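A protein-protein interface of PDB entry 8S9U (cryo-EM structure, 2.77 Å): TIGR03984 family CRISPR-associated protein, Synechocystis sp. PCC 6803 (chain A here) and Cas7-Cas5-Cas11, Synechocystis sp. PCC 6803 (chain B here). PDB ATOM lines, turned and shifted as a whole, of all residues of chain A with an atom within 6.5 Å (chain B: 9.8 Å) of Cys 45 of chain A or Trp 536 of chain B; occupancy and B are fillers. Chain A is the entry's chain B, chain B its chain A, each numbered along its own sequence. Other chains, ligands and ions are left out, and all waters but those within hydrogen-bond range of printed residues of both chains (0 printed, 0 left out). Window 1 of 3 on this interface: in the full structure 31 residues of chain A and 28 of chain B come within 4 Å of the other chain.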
ATOM      1  N   LEU A  38      11.336  -3.094 -19.023  1.00  0.00           N
ATOM      2  CA  LEU A  38      11.214  -4.536 -19.134  1.00  0.00           C
ATOM      3  C   LEU A  38      10.229  -4.820 -20.253  1.00  0.00           C
ATOM      4  O   LEU A  38       9.100  -4.327 -20.222  1.00  0.00           O
ATOM      5  CB  LEU A  38      10.733  -5.130 -17.812  1.00  0.00           C
ATOM      6  CG  LEU A  38      10.892  -6.618 -17.532  1.00  0.00           C
ATOM      7  CD1 LEU A  38      12.299  -7.065 -17.804  1.00  0.00           C
ATOM      8  CD2 LEU A  38      10.522  -6.890 -16.096  1.00  0.00           C
ATOM      9  N   LEU A  39      10.650  -5.609 -21.234  1.00  0.00           N
ATOM     10  CA  LEU A  39       9.863  -5.828 -22.440  1.00  0.00           C
ATOM     11  C   LEU A  39       9.526  -7.300 -22.545  1.00  0.00           C
ATOM     12  O   LEU A  39      10.424  -8.143 -22.572  1.00  0.00           O
ATOM     13  CB  LEU A  39      10.615  -5.377 -23.689  1.00  0.00           C
ATOM     14  CG  LEU A  39      11.290  -4.012 -23.695  1.00  0.00           C
ATOM     15  CD1 LEU A  39      12.061  -3.847 -24.974  1.00  0.00           C
ATOM     16  CD2 LEU A  39      10.280  -2.903 -23.544  1.00  0.00           C
ATOM     17  N   TYR A  40       8.239  -7.603 -22.607  1.00  0.00           N
ATOM     18  CA  TYR A  40       7.758  -8.969 -22.684  1.00  0.00           C
ATOM     19  C   TYR A  40       7.484  -9.308 -24.137  1.00  0.00           C
ATOM     20  O   TYR A  40       6.708  -8.624 -24.803  1.00  0.00           O
ATOM     21  CB  TYR A  40       6.498  -9.171 -21.851  1.00  0.00           C
ATOM     22  CG  TYR A  40       6.633  -8.872 -20.379  1.00  0.00           C
ATOM     23  CD1 TYR A  40       7.867  -8.782 -19.771  1.00  0.00           C
ATOM     24  CD2 TYR A  40       5.514  -8.706 -19.595  1.00  0.00           C
ATOM     25  CE1 TYR A  40       7.979  -8.517 -18.434  1.00  0.00           C
ATOM     26  CE2 TYR A  40       5.619  -8.445 -18.264  1.00  0.00           C
ATOM     27  CZ  TYR A  40       6.850  -8.351 -17.686  1.00  0.00           C
ATOM     28  OH  TYR A  40       6.942  -8.085 -16.344  1.00  0.00           O
ATOM     29  N   SER A  41       8.140 -10.341 -24.625  1.00  0.00           N
ATOM     30  CA  SER A  41       8.023 -10.827 -25.986  1.00  0.00           C
ATOM     31  C   SER A  41       7.861 -12.331 -25.889  1.00  0.00           C
ATOM     32  O   SER A  41       8.170 -12.921 -24.850  1.00  0.00           O
ATOM     33  CB  SER A  41       9.269 -10.452 -26.800  1.00  0.00           C
ATOM     34  OG  SER A  41       9.456 -11.303 -27.910  1.00  0.00           O
ATOM     35  N   PRO A  42       7.371 -12.986 -26.942  1.00  0.00           N
ATOM     36  CA  PRO A  42       7.094 -14.418 -26.825  1.00  0.00           C
ATOM     37  C   PRO A  42       8.305 -15.237 -26.463  1.00  0.00           C
ATOM     38  O   PRO A  42       8.163 -16.272 -25.807  1.00  0.00           O
ATOM     39  CB  PRO A  42       6.586 -14.766 -28.220  1.00  0.00           C
ATOM     40  CG  PRO A  42       5.851 -13.583 -28.602  1.00  0.00           C
ATOM     41  CD  PRO A  42       6.640 -12.413 -28.084  1.00  0.00           C
ATOM     42  N   GLN A  43       9.496 -14.796 -26.860  1.00  0.00           N
ATOM     43  CA  GLN A  43      10.715 -15.554 -26.652  1.00  0.00           C
ATOM     44  C   GLN A  43      11.702 -14.926 -25.687  1.00  0.00           C
ATOM     45  O   GLN A  43      12.636 -15.611 -25.270  1.00  0.00           O
ATOM     46  CB  GLN A  43      11.433 -15.745 -27.989  1.00  0.00           C
ATOM     47  CG  GLN A  43      10.820 -16.766 -28.884  1.00  0.00           C
ATOM     48  CD  GLN A  43      11.807 -17.825 -29.282  1.00  0.00           C
ATOM     49  OE1 GLN A  43      12.383 -17.763 -30.362  1.00  0.00           O
ATOM     50  NE2 GLN A  43      12.016 -18.803 -28.411  1.00  0.00           N
ATOM     51  N   LYS A  44      11.549 -13.661 -25.327  1.00  0.00           N
ATOM     52  CA  LYS A  44      12.471 -13.068 -24.376  1.00  0.00           C
ATOM     53  C   LYS A  44      11.782 -12.067 -23.468  1.00  0.00           C
ATOM     54  O   LYS A  44      10.771 -11.464 -23.825  1.00  0.00           O
ATOM     55  CB  LYS A  44      13.640 -12.387 -25.085  1.00  0.00           C
ATOM     56  CG  LYS A  44      13.260 -11.658 -26.340  1.00  0.00           C
ATOM     57  CD  LYS A  44      14.476 -11.078 -27.013  1.00  0.00           C
ATOM     58  CE  LYS A  44      14.085 -10.288 -28.242  1.00  0.00           C
ATOM     59  NZ  LYS A  44      15.237  -9.532 -28.800  1.00  0.00           N
ATOM     60  N   CYS A  45      12.357 -11.903 -22.284  1.00  0.00           N
ATOM     61  CA  CYS A  45      11.985 -10.886 -21.310  1.00  0.00           C
ATOM     62  C   CYS A  45      13.292 -10.121 -21.151  1.00  0.00           C
ATOM     63  O   CYS A  45      14.147 -10.483 -20.342  1.00  0.00           O
ATOM     64  CB  CYS A  45      11.497 -11.488 -20.012  1.00  0.00           C
ATOM     65  SG  CYS A  45      11.026 -10.316 -18.758  1.00  0.00           S
ATOM     66  N   GLU A  46      13.439  -9.058 -21.928  1.00  0.00           N
ATOM     67  CA  GLU A  46      14.660  -8.272 -21.961  1.00  0.00           C
ATOM     68  C   GLU A  46      14.540  -6.979 -21.174  1.00  0.00           C
ATOM     69  O   GLU A  46      13.513  -6.299 -21.217  1.00  0.00           O
ATOM     70  CB  GLU A  46      15.044  -7.956 -23.402  1.00  0.00           C
ATOM     71  CG  GLU A  46      13.877  -7.924 -24.342  1.00  0.00           C
ATOM     72  CD  GLU A  46      14.278  -7.485 -25.724  1.00  0.00           C
ATOM     73  OE1 GLU A  46      13.384  -7.129 -26.519  1.00  0.00           O
ATOM     74  OE2 GLU A  46      15.492  -7.498 -26.017  1.00  0.00           O
ATOM     75  N   LEU A  47      15.609  -6.646 -20.462  1.00  0.00           N
ATOM     76  CA  LEU A  47      15.716  -5.413 -19.701  1.00  0.00           C
ATOM     77  C   LEU A  47      16.427  -4.385 -20.564  1.00  0.00           C
ATOM     78  O   LEU A  47      17.429  -4.702 -21.209  1.00  0.00           O
ATOM     79  CB  LEU A  47      16.506  -5.637 -18.414  1.00  0.00           C
ATOM     80  CG  LEU A  47      15.780  -5.975 -17.119  1.00  0.00           C
ATOM     81  CD1 LEU A  47      16.773  -6.513 -16.124  1.00  0.00           C
ATOM     82  CD2 LEU A  47      15.096  -4.752 -16.565  1.00  0.00           C
ATOM     83  N   PHE A  71       4.781  -7.529 -26.705  1.00  0.00           N
ATOM     84  CA  PHE A  71       3.354  -7.434 -26.454  1.00  0.00           C
ATOM     85  C   PHE A  71       3.028  -6.677 -25.181  1.00  0.00           C
ATOM     86  O   PHE A  71       1.895  -6.221 -25.023  1.00  0.00           O
ATOM     87  CB  PHE A  71       2.716  -8.824 -26.416  1.00  0.00           C
ATOM     88  CG  PHE A  71       3.232  -9.723 -25.336  1.00  0.00           C
ATOM     89  CD1 PHE A  71       2.800  -9.605 -24.034  1.00  0.00           C
ATOM     90  CD2 PHE A  71       4.085 -10.748 -25.646  1.00  0.00           C
ATOM     91  CE1 PHE A  71       3.260 -10.451 -23.067  1.00  0.00           C
ATOM     92  CE2 PHE A  71       4.536 -11.599 -24.680  1.00  0.00           C
ATOM     93  CZ  PHE A  71       4.125 -11.449 -23.391  1.00  0.00           C
ATOM     94  N   LEU A 149      21.758 -13.040 -15.703  1.00  0.00           N
ATOM     95  CA  LEU A 149      20.785 -11.962 -15.834  1.00  0.00           C
ATOM     96  C   LEU A 149      21.559 -10.656 -15.912  1.00  0.00           C
ATOM     97  O   LEU A 149      22.283 -10.314 -14.974  1.00  0.00           O
ATOM     98  CB  LEU A 149      19.811 -11.946 -14.654  1.00  0.00           C
ATOM     99  CG  LEU A 149      18.811 -10.794 -14.560  1.00  0.00           C
ATOM    100  CD1 LEU A 149      17.886 -10.780 -15.752  1.00  0.00           C
ATOM    101  CD2 LEU A 149      18.018 -10.884 -13.285  1.00  0.00           C
ATOM    102  N   GLU B  90      22.980 -20.946 -18.927  1.00  0.00           N
ATOM    103  CA  GLU B  90      21.692 -21.557 -18.640  1.00  0.00           C
ATOM    104  C   GLU B  90      21.837 -23.069 -18.503  1.00  0.00           C
ATOM    105  O   GLU B  90      22.640 -23.683 -19.211  1.00  0.00           O
ATOM    106  CB  GLU B  90      20.687 -21.216 -19.738  1.00  0.00           C
ATOM    107  CG  GLU B  90      20.439 -19.727 -19.888  1.00  0.00           C
ATOM    108  CD  GLU B  90      21.350 -19.072 -20.912  1.00  0.00           C
ATOM    109  OE1 GLU B  90      20.896 -18.133 -21.601  1.00  0.00           O
ATOM    110  OE2 GLU B  90      22.521 -19.494 -21.026  1.00  0.00           O
ATOM    111  N   PRO B  91      21.096 -23.695 -17.593  1.00  0.00           N
ATOM    112  CA  PRO B  91      21.223 -25.144 -17.397  1.00  0.00           C
ATOM    113  C   PRO B  91      20.740 -25.940 -18.601  1.00  0.00           C
ATOM    114  O   PRO B  91      19.629 -25.740 -19.091  1.00  0.00           O
ATOM    115  CB  PRO B  91      20.362 -25.404 -16.158  1.00  0.00           C
ATOM    116  CG  PRO B  91      19.412 -24.296 -16.117  1.00  0.00           C
ATOM    117  CD  PRO B  91      20.095 -23.107 -16.693  1.00  0.00           C
ATOM    118  N   GLN B 229      18.532 -23.114 -27.296  1.00  0.00           N
ATOM    119  CA  GLN B 229      17.107 -23.335 -27.481  1.00  0.00           C
ATOM    120  C   GLN B 229      16.772 -23.501 -28.957  1.00  0.00           C
ATOM    121  O   GLN B 229      17.437 -22.948 -29.835  1.00  0.00           O
ATOM    122  CB  GLN B 229      16.306 -22.178 -26.888  1.00  0.00           C
ATOM    123  CG  GLN B 229      16.441 -22.025 -25.387  1.00  0.00           C
ATOM    124  CD  GLN B 229      15.642 -20.851 -24.853  1.00  0.00           C
ATOM    125  OE1 GLN B 229      14.751 -20.336 -25.526  1.00  0.00           O
ATOM    126  NE2 GLN B 229      15.960 -20.418 -23.638  1.00  0.00           N
ATOM    127  N   ASN B 230      15.731 -24.278 -29.228  1.00  0.00           N
ATOM    128  CA  ASN B 230      15.001 -24.168 -30.487  1.00  0.00           C
ATOM    129  C   ASN B 230      14.137 -22.916 -30.445  1.00  0.00           C
ATOM    130  O   ASN B 230      13.028 -22.927 -29.910  1.00  0.00           O
ATOM    131  CB  ASN B 230      14.163 -25.414 -30.735  1.00  0.00           C
ATOM    132  CG  ASN B 230      15.011 -26.649 -30.950  1.00  0.00           C
ATOM    133  OD1 ASN B 230      15.802 -26.713 -31.889  1.00  0.00           O
ATOM    134  ND2 ASN B 230      14.842 -27.643 -30.087  1.00  0.00           N
ATOM    135  N   LYS B 231      14.657 -21.823 -30.988  1.00  0.00           N
ATOM    136  CA  LYS B 231      13.941 -20.561 -31.014  1.00  0.00           C
ATOM    137  C   LYS B 231      12.754 -20.616 -31.974  1.00  0.00           C
ATOM    138  O   LYS B 231      12.665 -21.478 -32.849  1.00  0.00           O
ATOM    139  CB  LYS B 231      14.891 -19.430 -31.387  1.00  0.00           C
ATOM    140  CG  LYS B 231      15.906 -19.154 -30.301  1.00  0.00           C
ATOM    141  CD  LYS B 231      16.371 -17.720 -30.319  1.00  0.00           C
ATOM    142  CE  LYS B 231      17.446 -17.489 -29.277  1.00  0.00           C
ATOM    143  NZ  LYS B 231      18.396 -16.414 -29.678  1.00  0.00           N
ATOM    144  N   LEU B 232      11.826 -19.680 -31.789  1.00  0.00           N
ATOM    145  CA  LEU B 232      10.636 -19.592 -32.623  1.00  0.00           C
ATOM    146  C   LEU B 232      10.892 -18.703 -33.826  1.00  0.00           C
ATOM    147  O   LEU B 232      11.627 -17.718 -33.753  1.00  0.00           O
ATOM    148  CB  LEU B 232       9.448 -19.012 -31.856  1.00  0.00           C
ATOM    149  CG  LEU B 232       8.748 -19.691 -30.691  1.00  0.00           C
ATOM    150  CD1 LEU B 232       7.917 -18.663 -29.966  1.00  0.00           C
ATOM    151  CD2 LEU B 232       7.881 -20.803 -31.194  1.00  0.00           C
ATOM    152  N   ARG B 486      -7.266  -7.031 -16.531  1.00  0.00           N
ATOM    153  CA  ARG B 486      -6.419  -5.965 -16.029  1.00  0.00           C
ATOM    154  C   ARG B 486      -7.270  -4.799 -15.560  1.00  0.00           C
ATOM    155  O   ARG B 486      -8.291  -4.476 -16.170  1.00  0.00           O
ATOM    156  CB  ARG B 486      -5.444  -5.495 -17.101  1.00  0.00           C
ATOM    157  CG  ARG B 486      -4.456  -6.545 -17.491  1.00  0.00           C
ATOM    158  CD  ARG B 486      -3.625  -6.111 -18.655  1.00  0.00           C
ATOM    159  NE  ARG B 486      -2.729  -7.176 -19.076  1.00  0.00           N
ATOM    160  CZ  ARG B 486      -1.453  -7.252 -18.728  1.00  0.00           C
ATOM    161  NH1 ARG B 486      -0.947  -6.378 -17.877  1.00  0.00           N
ATOM    162  NH2 ARG B 486      -0.705  -8.248 -19.170  1.00  0.00           N
ATOM    163  N   SER B 531       3.887 -19.029 -12.672  1.00  0.00           N
ATOM    164  CA  SER B 531       4.287 -19.936 -13.727  1.00  0.00           C
ATOM    165  C   SER B 531       5.653 -19.533 -14.245  1.00  0.00           C
ATOM    166  O   SER B 531       6.093 -18.397 -14.078  1.00  0.00           O
ATOM    167  CB  SER B 531       3.252 -19.933 -14.851  1.00  0.00           C
ATOM    168  OG  SER B 531       3.644 -20.775 -15.913  1.00  0.00           O
ATOM    169  N   TRP B 532       6.321 -20.486 -14.872  1.00  0.00           N
ATOM    170  CA  TRP B 532       7.589 -20.254 -15.535  1.00  0.00           C
ATOM    171  C   TRP B 532       7.371 -20.171 -17.036  1.00  0.00           C
ATOM    172  O   TRP B 532       6.465 -20.801 -17.580  1.00  0.00           O
ATOM    173  CB  TRP B 532       8.559 -21.383 -15.222  1.00  0.00           C
ATOM    174  CG  TRP B 532       9.978 -21.081 -15.510  1.00  0.00           C
ATOM    175  CD1 TRP B 532      10.654 -21.332 -16.654  1.00  0.00           C
ATOM    176  CD2 TRP B 532      10.916 -20.519 -14.606  1.00  0.00           C
ATOM    177  NE1 TRP B 532      11.950 -20.941 -16.531  1.00  0.00           N
ATOM    178  CE2 TRP B 532      12.137 -20.437 -15.274  1.00  0.00           C
ATOM    179  CE3 TRP B 532      10.839 -20.076 -13.289  1.00  0.00           C
ATOM    180  CZ2 TRP B 532      13.271 -19.933 -14.673  1.00  0.00           C
ATOM    181  CZ3 TRP B 532      11.957 -19.572 -12.704  1.00  0.00           C
ATOM    182  CH2 TRP B 532      13.158 -19.505 -13.388  1.00  0.00           C
ATOM    183  N   GLN B 533       8.197 -19.391 -17.708  1.00  0.00           N
ATOM    184  CA  GLN B 533       8.198 -19.374 -19.160  1.00  0.00           C
ATOM    185  C   GLN B 533       9.494 -19.978 -19.655  1.00  0.00           C
ATOM    186  O   GLN B 533      10.569 -19.424 -19.428  1.00  0.00           O
ATOM    187  CB  GLN B 533       8.017 -17.988 -19.743  1.00  0.00           C
ATOM    188  CG  GLN B 533       8.207 -18.062 -21.229  1.00  0.00           C
ATOM    189  CD  GLN B 533       7.315 -17.158 -21.958  1.00  0.00           C
ATOM    190  OE1 GLN B 533       6.533 -16.446 -21.355  1.00  0.00           O
ATOM    191  NE2 GLN B 533       7.403 -17.171 -23.270  1.00  0.00           N
ATOM    192  N   VAL B 534       9.383 -21.121 -20.326  1.00  0.00           N
ATOM    193  CA  VAL B 534      10.552 -21.874 -20.746  1.00  0.00           C
ATOM    194  C   VAL B 534      11.332 -21.121 -21.810  1.00  0.00           C
ATOM    195  O   VAL B 534      12.549 -21.294 -21.931  1.00  0.00           O
ATOM    196  CB  VAL B 534      10.103 -23.260 -21.216  1.00  0.00           C
ATOM    197  CG1 VAL B 534      11.269 -24.079 -21.642  1.00  0.00           C
ATOM    198  CG2 VAL B 534       9.371 -23.939 -20.099  1.00  0.00           C
ATOM    199  N   ARG B 535      10.671 -20.265 -22.580  1.00  0.00           N
ATOM    200  CA  ARG B 535      11.363 -19.531 -23.627  1.00  0.00           C
ATOM    201  C   ARG B 535      12.079 -18.315 -23.081  1.00  0.00           C
ATOM    202  O   ARG B 535      12.996 -17.809 -23.727  1.00  0.00           O
ATOM    203  CB  ARG B 535      10.392 -19.098 -24.717  1.00  0.00           C
ATOM    204  CG  ARG B 535       9.627 -20.231 -25.336  1.00  0.00           C
ATOM    205  CD  ARG B 535       8.958 -19.798 -26.610  1.00  0.00           C
ATOM    206  NE  ARG B 535       8.101 -20.843 -27.136  1.00  0.00           N
ATOM    207  CZ  ARG B 535       8.527 -21.864 -27.862  1.00  0.00           C
ATOM    208  NH1 ARG B 535       9.806 -21.978 -28.162  1.00  0.00           N
ATOM    209  NH2 ARG B 535       7.670 -22.770 -28.294  1.00  0.00           N
ATOM    210  N   TRP B 536      11.694 -17.858 -21.900  1.00  0.00           N
ATOM    211  CA  TRP B 536      12.324 -16.726 -21.248  1.00  0.00           C
ATOM    212  C   TRP B 536      13.429 -17.150 -20.307  1.00  0.00           C
ATOM    213  O   TRP B 536      14.330 -16.354 -20.031  1.00  0.00           O
ATOM    214  CB  TRP B 536      11.310 -15.941 -20.415  1.00  0.00           C
ATOM    215  CG  TRP B 536      10.307 -15.166 -21.150  1.00  0.00           C
ATOM    216  CD1 TRP B 536      10.127 -15.124 -22.483  1.00  0.00           C
ATOM    217  CD2 TRP B 536       9.338 -14.286 -20.584  1.00  0.00           C
ATOM    218  NE1 TRP B 536       9.101 -14.274 -22.797  1.00  0.00           N
ATOM    219  CE2 TRP B 536       8.601 -13.745 -21.641  1.00  0.00           C
ATOM    220  CE3 TRP B 536       9.021 -13.906 -19.282  1.00  0.00           C
ATOM    221  CZ2 TRP B 536       7.570 -12.847 -21.441  1.00  0.00           C
ATOM    222  CZ3 TRP B 536       8.004 -13.019 -19.089  1.00  0.00           C
ATOM    223  CH2 TRP B 536       7.288 -12.500 -20.158  1.00  0.00           C
ATOM    224  N   GLY B 537      13.388 -18.386 -19.826  1.00  0.00           N
ATOM    225  CA  GLY B 537      14.287 -18.811 -18.778  1.00  0.00           C
ATOM    226  C   GLY B 537      14.063 -18.040 -17.504  1.00  0.00           C
ATOM    227  O   GLY B 537      14.968 -17.935 -16.674  1.00  0.00           O
ATOM    228  N   LEU B 538      12.864 -17.511 -17.326  1.00  0.00           N
ATOM    229  CA  LEU B 538      12.476 -16.690 -16.195  1.00  0.00           C
ATOM    230  C   LEU B 538      11.028 -17.014 -15.892  1.00  0.00           C
ATOM    231  O   LEU B 538      10.300 -17.481 -16.771  1.00  0.00           O
ATOM    232  CB  LEU B 538      12.623 -15.198 -16.504  1.00  0.00           C
ATOM    233  CG  LEU B 538      14.032 -14.653 -16.650  1.00  0.00           C
ATOM    234  CD1 LEU B 538      13.959 -13.216 -17.056  1.00  0.00           C
ATOM    235  CD2 LEU B 538      14.755 -14.793 -15.348  1.00  0.00           C
ATOM    236  N   PRO B 539      10.582 -16.799 -14.663  1.00  0.00           N
ATOM    237  CA  PRO B 539       9.160 -16.956 -14.382  1.00  0.00           C
ATOM    238  C   PRO B 539       8.343 -15.965 -15.182  1.00  0.00           C
ATOM    239  O   PRO B 539       8.809 -14.879 -15.526  1.00  0.00           O
ATOM    240  CB  PRO B 539       9.070 -16.703 -12.879  1.00  0.00           C
ATOM    241  CG  PRO B 539      10.180 -15.864 -12.593  1.00  0.00           C
ATOM    242  CD  PRO B 539      11.291 -16.284 -13.486  1.00  0.00           C
ATOM    243  N   ARG B 540       7.125 -16.355 -15.499  1.00  0.00           N
ATOM    244  CA  ARG B 540       6.200 -15.408 -16.089  1.00  0.00           C
ATOM    245  C   ARG B 540       5.951 -14.325 -15.058  1.00  0.00           C
ATOM    246  O   ARG B 540       6.370 -14.462 -13.906  1.00  0.00           O
ATOM    247  CB  ARG B 540       4.893 -16.101 -16.458  1.00  0.00           C
ATOM    248  CG  ARG B 540       5.012 -17.166 -17.505  1.00  0.00           C
ATOM    249  CD  ARG B 540       3.704 -17.893 -17.660  1.00  0.00           C
ATOM    250  NE  ARG B 540       2.684 -17.190 -18.403  1.00  0.00           N
ATOM    251  CZ  ARG B 540       1.494 -17.708 -18.665  1.00  0.00           C
ATOM    252  NH1 ARG B 540       1.146 -18.857 -18.125  1.00  0.00           N
ATOM    253  NH2 ARG B 540       0.612 -17.028 -19.367  1.00  0.00           N
ATOM    254  N   PRO B 541       5.253 -13.270 -15.393  1.00  0.00           N
ATOM    255  CA  PRO B 541       4.788 -12.378 -14.341  1.00  0.00           C
ATOM    256  C   PRO B 541       3.756 -13.125 -13.532  1.00  0.00           C
ATOM    257  O   PRO B 541       3.517 -14.307 -13.781  1.00  0.00           O
ATOM    258  CB  PRO B 541       4.186 -11.208 -15.124  1.00  0.00           C
ATOM    259  CG  PRO B 541       3.942 -11.784 -16.470  1.00  0.00           C
ATOM    260  CD  PRO B 541       5.147 -12.595 -16.688  1.00  0.00           C
ATOM    261  N   SER B 542       3.108 -12.480 -12.586  1.00  0.00           N
ATOM    262  CA  SER B 542       2.121 -13.174 -11.789  1.00  0.00           C
ATOM    263  C   SER B 542       0.773 -12.765 -12.335  1.00  0.00           C
ATOM    264  O   SER B 542       0.527 -11.580 -12.568  1.00  0.00           O
ATOM    265  CB  SER B 542       2.252 -12.825 -10.312  1.00  0.00           C
ATOM    266  OG  SER B 542       1.458 -13.682  -9.523  1.00  0.00           O
ATOM    267  N   LEU B 543      -0.089 -13.743 -12.550  1.00  0.00           N
ATOM    268  CA  LEU B 543      -1.365 -13.527 -13.209  1.00  0.00           C
ATOM    269  C   LEU B 543      -2.450 -13.688 -12.166  1.00  0.00           C
ATOM    270  O   LEU B 543      -2.662 -14.787 -11.647  1.00  0.00           O
ATOM    271  CB  LEU B 543      -1.562 -14.508 -14.358  1.00  0.00           C
ATOM    272  CG  LEU B 543      -0.460 -14.562 -15.411  1.00  0.00           C
ATOM    273  CD1 LEU B 543      -0.761 -15.636 -16.419  1.00  0.00           C
ATOM    274  CD2 LEU B 543      -0.282 -13.231 -16.075  1.00  0.00           C
ATOM    275  N   ARG B 577      -4.738 -13.159 -22.187  1.00  0.00           N
ATOM    276  CA  ARG B 577      -4.196 -14.496 -22.425  1.00  0.00           C
ATOM    277  C   ARG B 577      -5.272 -15.545 -22.663  1.00  0.00           C
ATOM    278  O   ARG B 577      -5.168 -16.679 -22.204  1.00  0.00           O
ATOM    279  CB  ARG B 577      -3.238 -14.919 -21.315  1.00  0.00           C
ATOM    280  CG  ARG B 577      -1.971 -14.110 -21.345  1.00  0.00           C
ATOM    281  CD  ARG B 577      -1.052 -14.382 -20.202  1.00  0.00           C
ATOM    282  NE  ARG B 577      -0.524 -13.153 -19.643  1.00  0.00           N
ATOM    283  CZ  ARG B 577       0.753 -12.808 -19.707  1.00  0.00           C
ATOM    284  NH1 ARG B 577       1.630 -13.640 -20.226  1.00  0.00           N
ATOM    285  NH2 ARG B 577       1.165 -11.668 -19.186  1.00  0.00           N
ATOM    286  N   GLU B 580      -4.336 -18.995 -24.197  1.00  0.00           N
ATOM    287  CA  GLU B 580      -3.942 -20.104 -23.345  1.00  0.00           C
ATOM    288  C   GLU B 580      -5.107 -20.814 -22.690  1.00  0.00           C
ATOM    289  O   GLU B 580      -4.889 -21.813 -22.004  1.00  0.00           O
ATOM    290  CB  GLU B 580      -3.003 -19.609 -22.258  1.00  0.00           C
ATOM    291  CG  GLU B 580      -1.669 -19.172 -22.750  1.00  0.00           C
ATOM    292  CD  GLU B 580      -0.958 -18.345 -21.729  1.00  0.00           C
ATOM    293  OE1 GLU B 580      -0.827 -17.128 -21.946  1.00  0.00           O
ATOM    294  OE2 GLU B 580      -0.547 -18.900 -20.697  1.00  0.00           O
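The indole nitrogen (NE1) of Trp 536 of chain B lies within hydrogen-bond range of the backbone carbonyl oxygen (O) of Lys 44 of chain A (3.4 Å). The backbone carbonyl oxygen of Arg 535 of chain B lies close to the backbone carbonyl oxygen of Gln 43 of chain A. The side-chain amide nitrogen (NE2) of Gln 533 of chain B sits at hydrogen-bond distance from the backbone carbonyl oxygen (O) of Pro 42 of chain A (2.8 Å). The backbone NH (N) of Leu 232 of chain B is in hydrogen-bond range of the side-chain amide oxygen (OE1) of Gln 43 of chain A (2.5 Å). O of Ser 41 of chain A is in hydrogen-bond range of NE1 of Trp 536 of chain B, 2.6 Å away.
OE2 of Glu 46 of chain A is in salt-bridge range of NZ of Lys 44 of chain A, at 3.5 Å. NE1 of Trp 536 of chain B sits close to NE2 of Gln 533 of chain B (3.4 Å). O of Leu 538 of chain B sits at hydrogen-bond distance from N of Gln 533 of chain B, 3.0 Å away. The backbone carbonyl oxygen (O) of Tyr 40 of chain A lies within hydrogen-bond range of the backbone NH (N) of Phe 71 of chain A (2.9 Å).
Among the printed residues, merely in contact across the chains: Tyr 40 of chain A with Trp 536 of chain B (3.7 Å), Pro 42 of chain A with Arg 535 of chain B (3.7 Å), Pro 42 of chain A with Trp 536 of chain B (3.7 Å), Gln 43 of chain A with Lys 231 of chain B (3.2 Å), Gln 43 of chain A with Trp 536 of chain B (3.6 Å) and Cys 45 of chain A with Trp 536 of chain B (3.5 Å).
Tyr 40 of chain A touches just one residue of chain B: Trp 536 (3.7 Å). Printed residues of chain B within 4 Å of Lys 44 of chain A: Trp 536 (3.4 Å). Cys 45 of chain A touches just one residue of chain B: Trp 536. Glu 90 of chain B touches none of the printed residues of chain A. Arg 486 of chain B touches none of the printed residues of chain A. Of the printed residues of chain A, Gln 533 of chain B touches Pro 42. Printed residues of chain A within 4 Å of Arg 535 of chain B: Pro 42 (3.7 Å) and Gln 43 (2.7 Å). Trp 536 of chain B touches just these residues of chain A: Tyr 40, Ser 41, Pro 42, Gln 43, Lys 44 and Cys 45. The nearest residue of chain B that does not touch Cys 45 of chain A is Leu 538 of chain B (4.2 Å).
Hydrophobic or aromatic side chains of chain B within 4 Å of the printed part of chain A: Leu 232 and Trp 536. Of the 12 printed residues of chain A, 6 touch a printed residue of chain B. Printed residues of chain A that touch a printed residue of chain B: Tyr 40, Ser 41, Pro 42, Gln 43, Lys 44 and Cys 45. Hydrophobic or aromatic side chains of chain A within 4 Å of the printed part of chain B: Tyr 40. Among the printed residues, 11 pairs touch across the chains.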
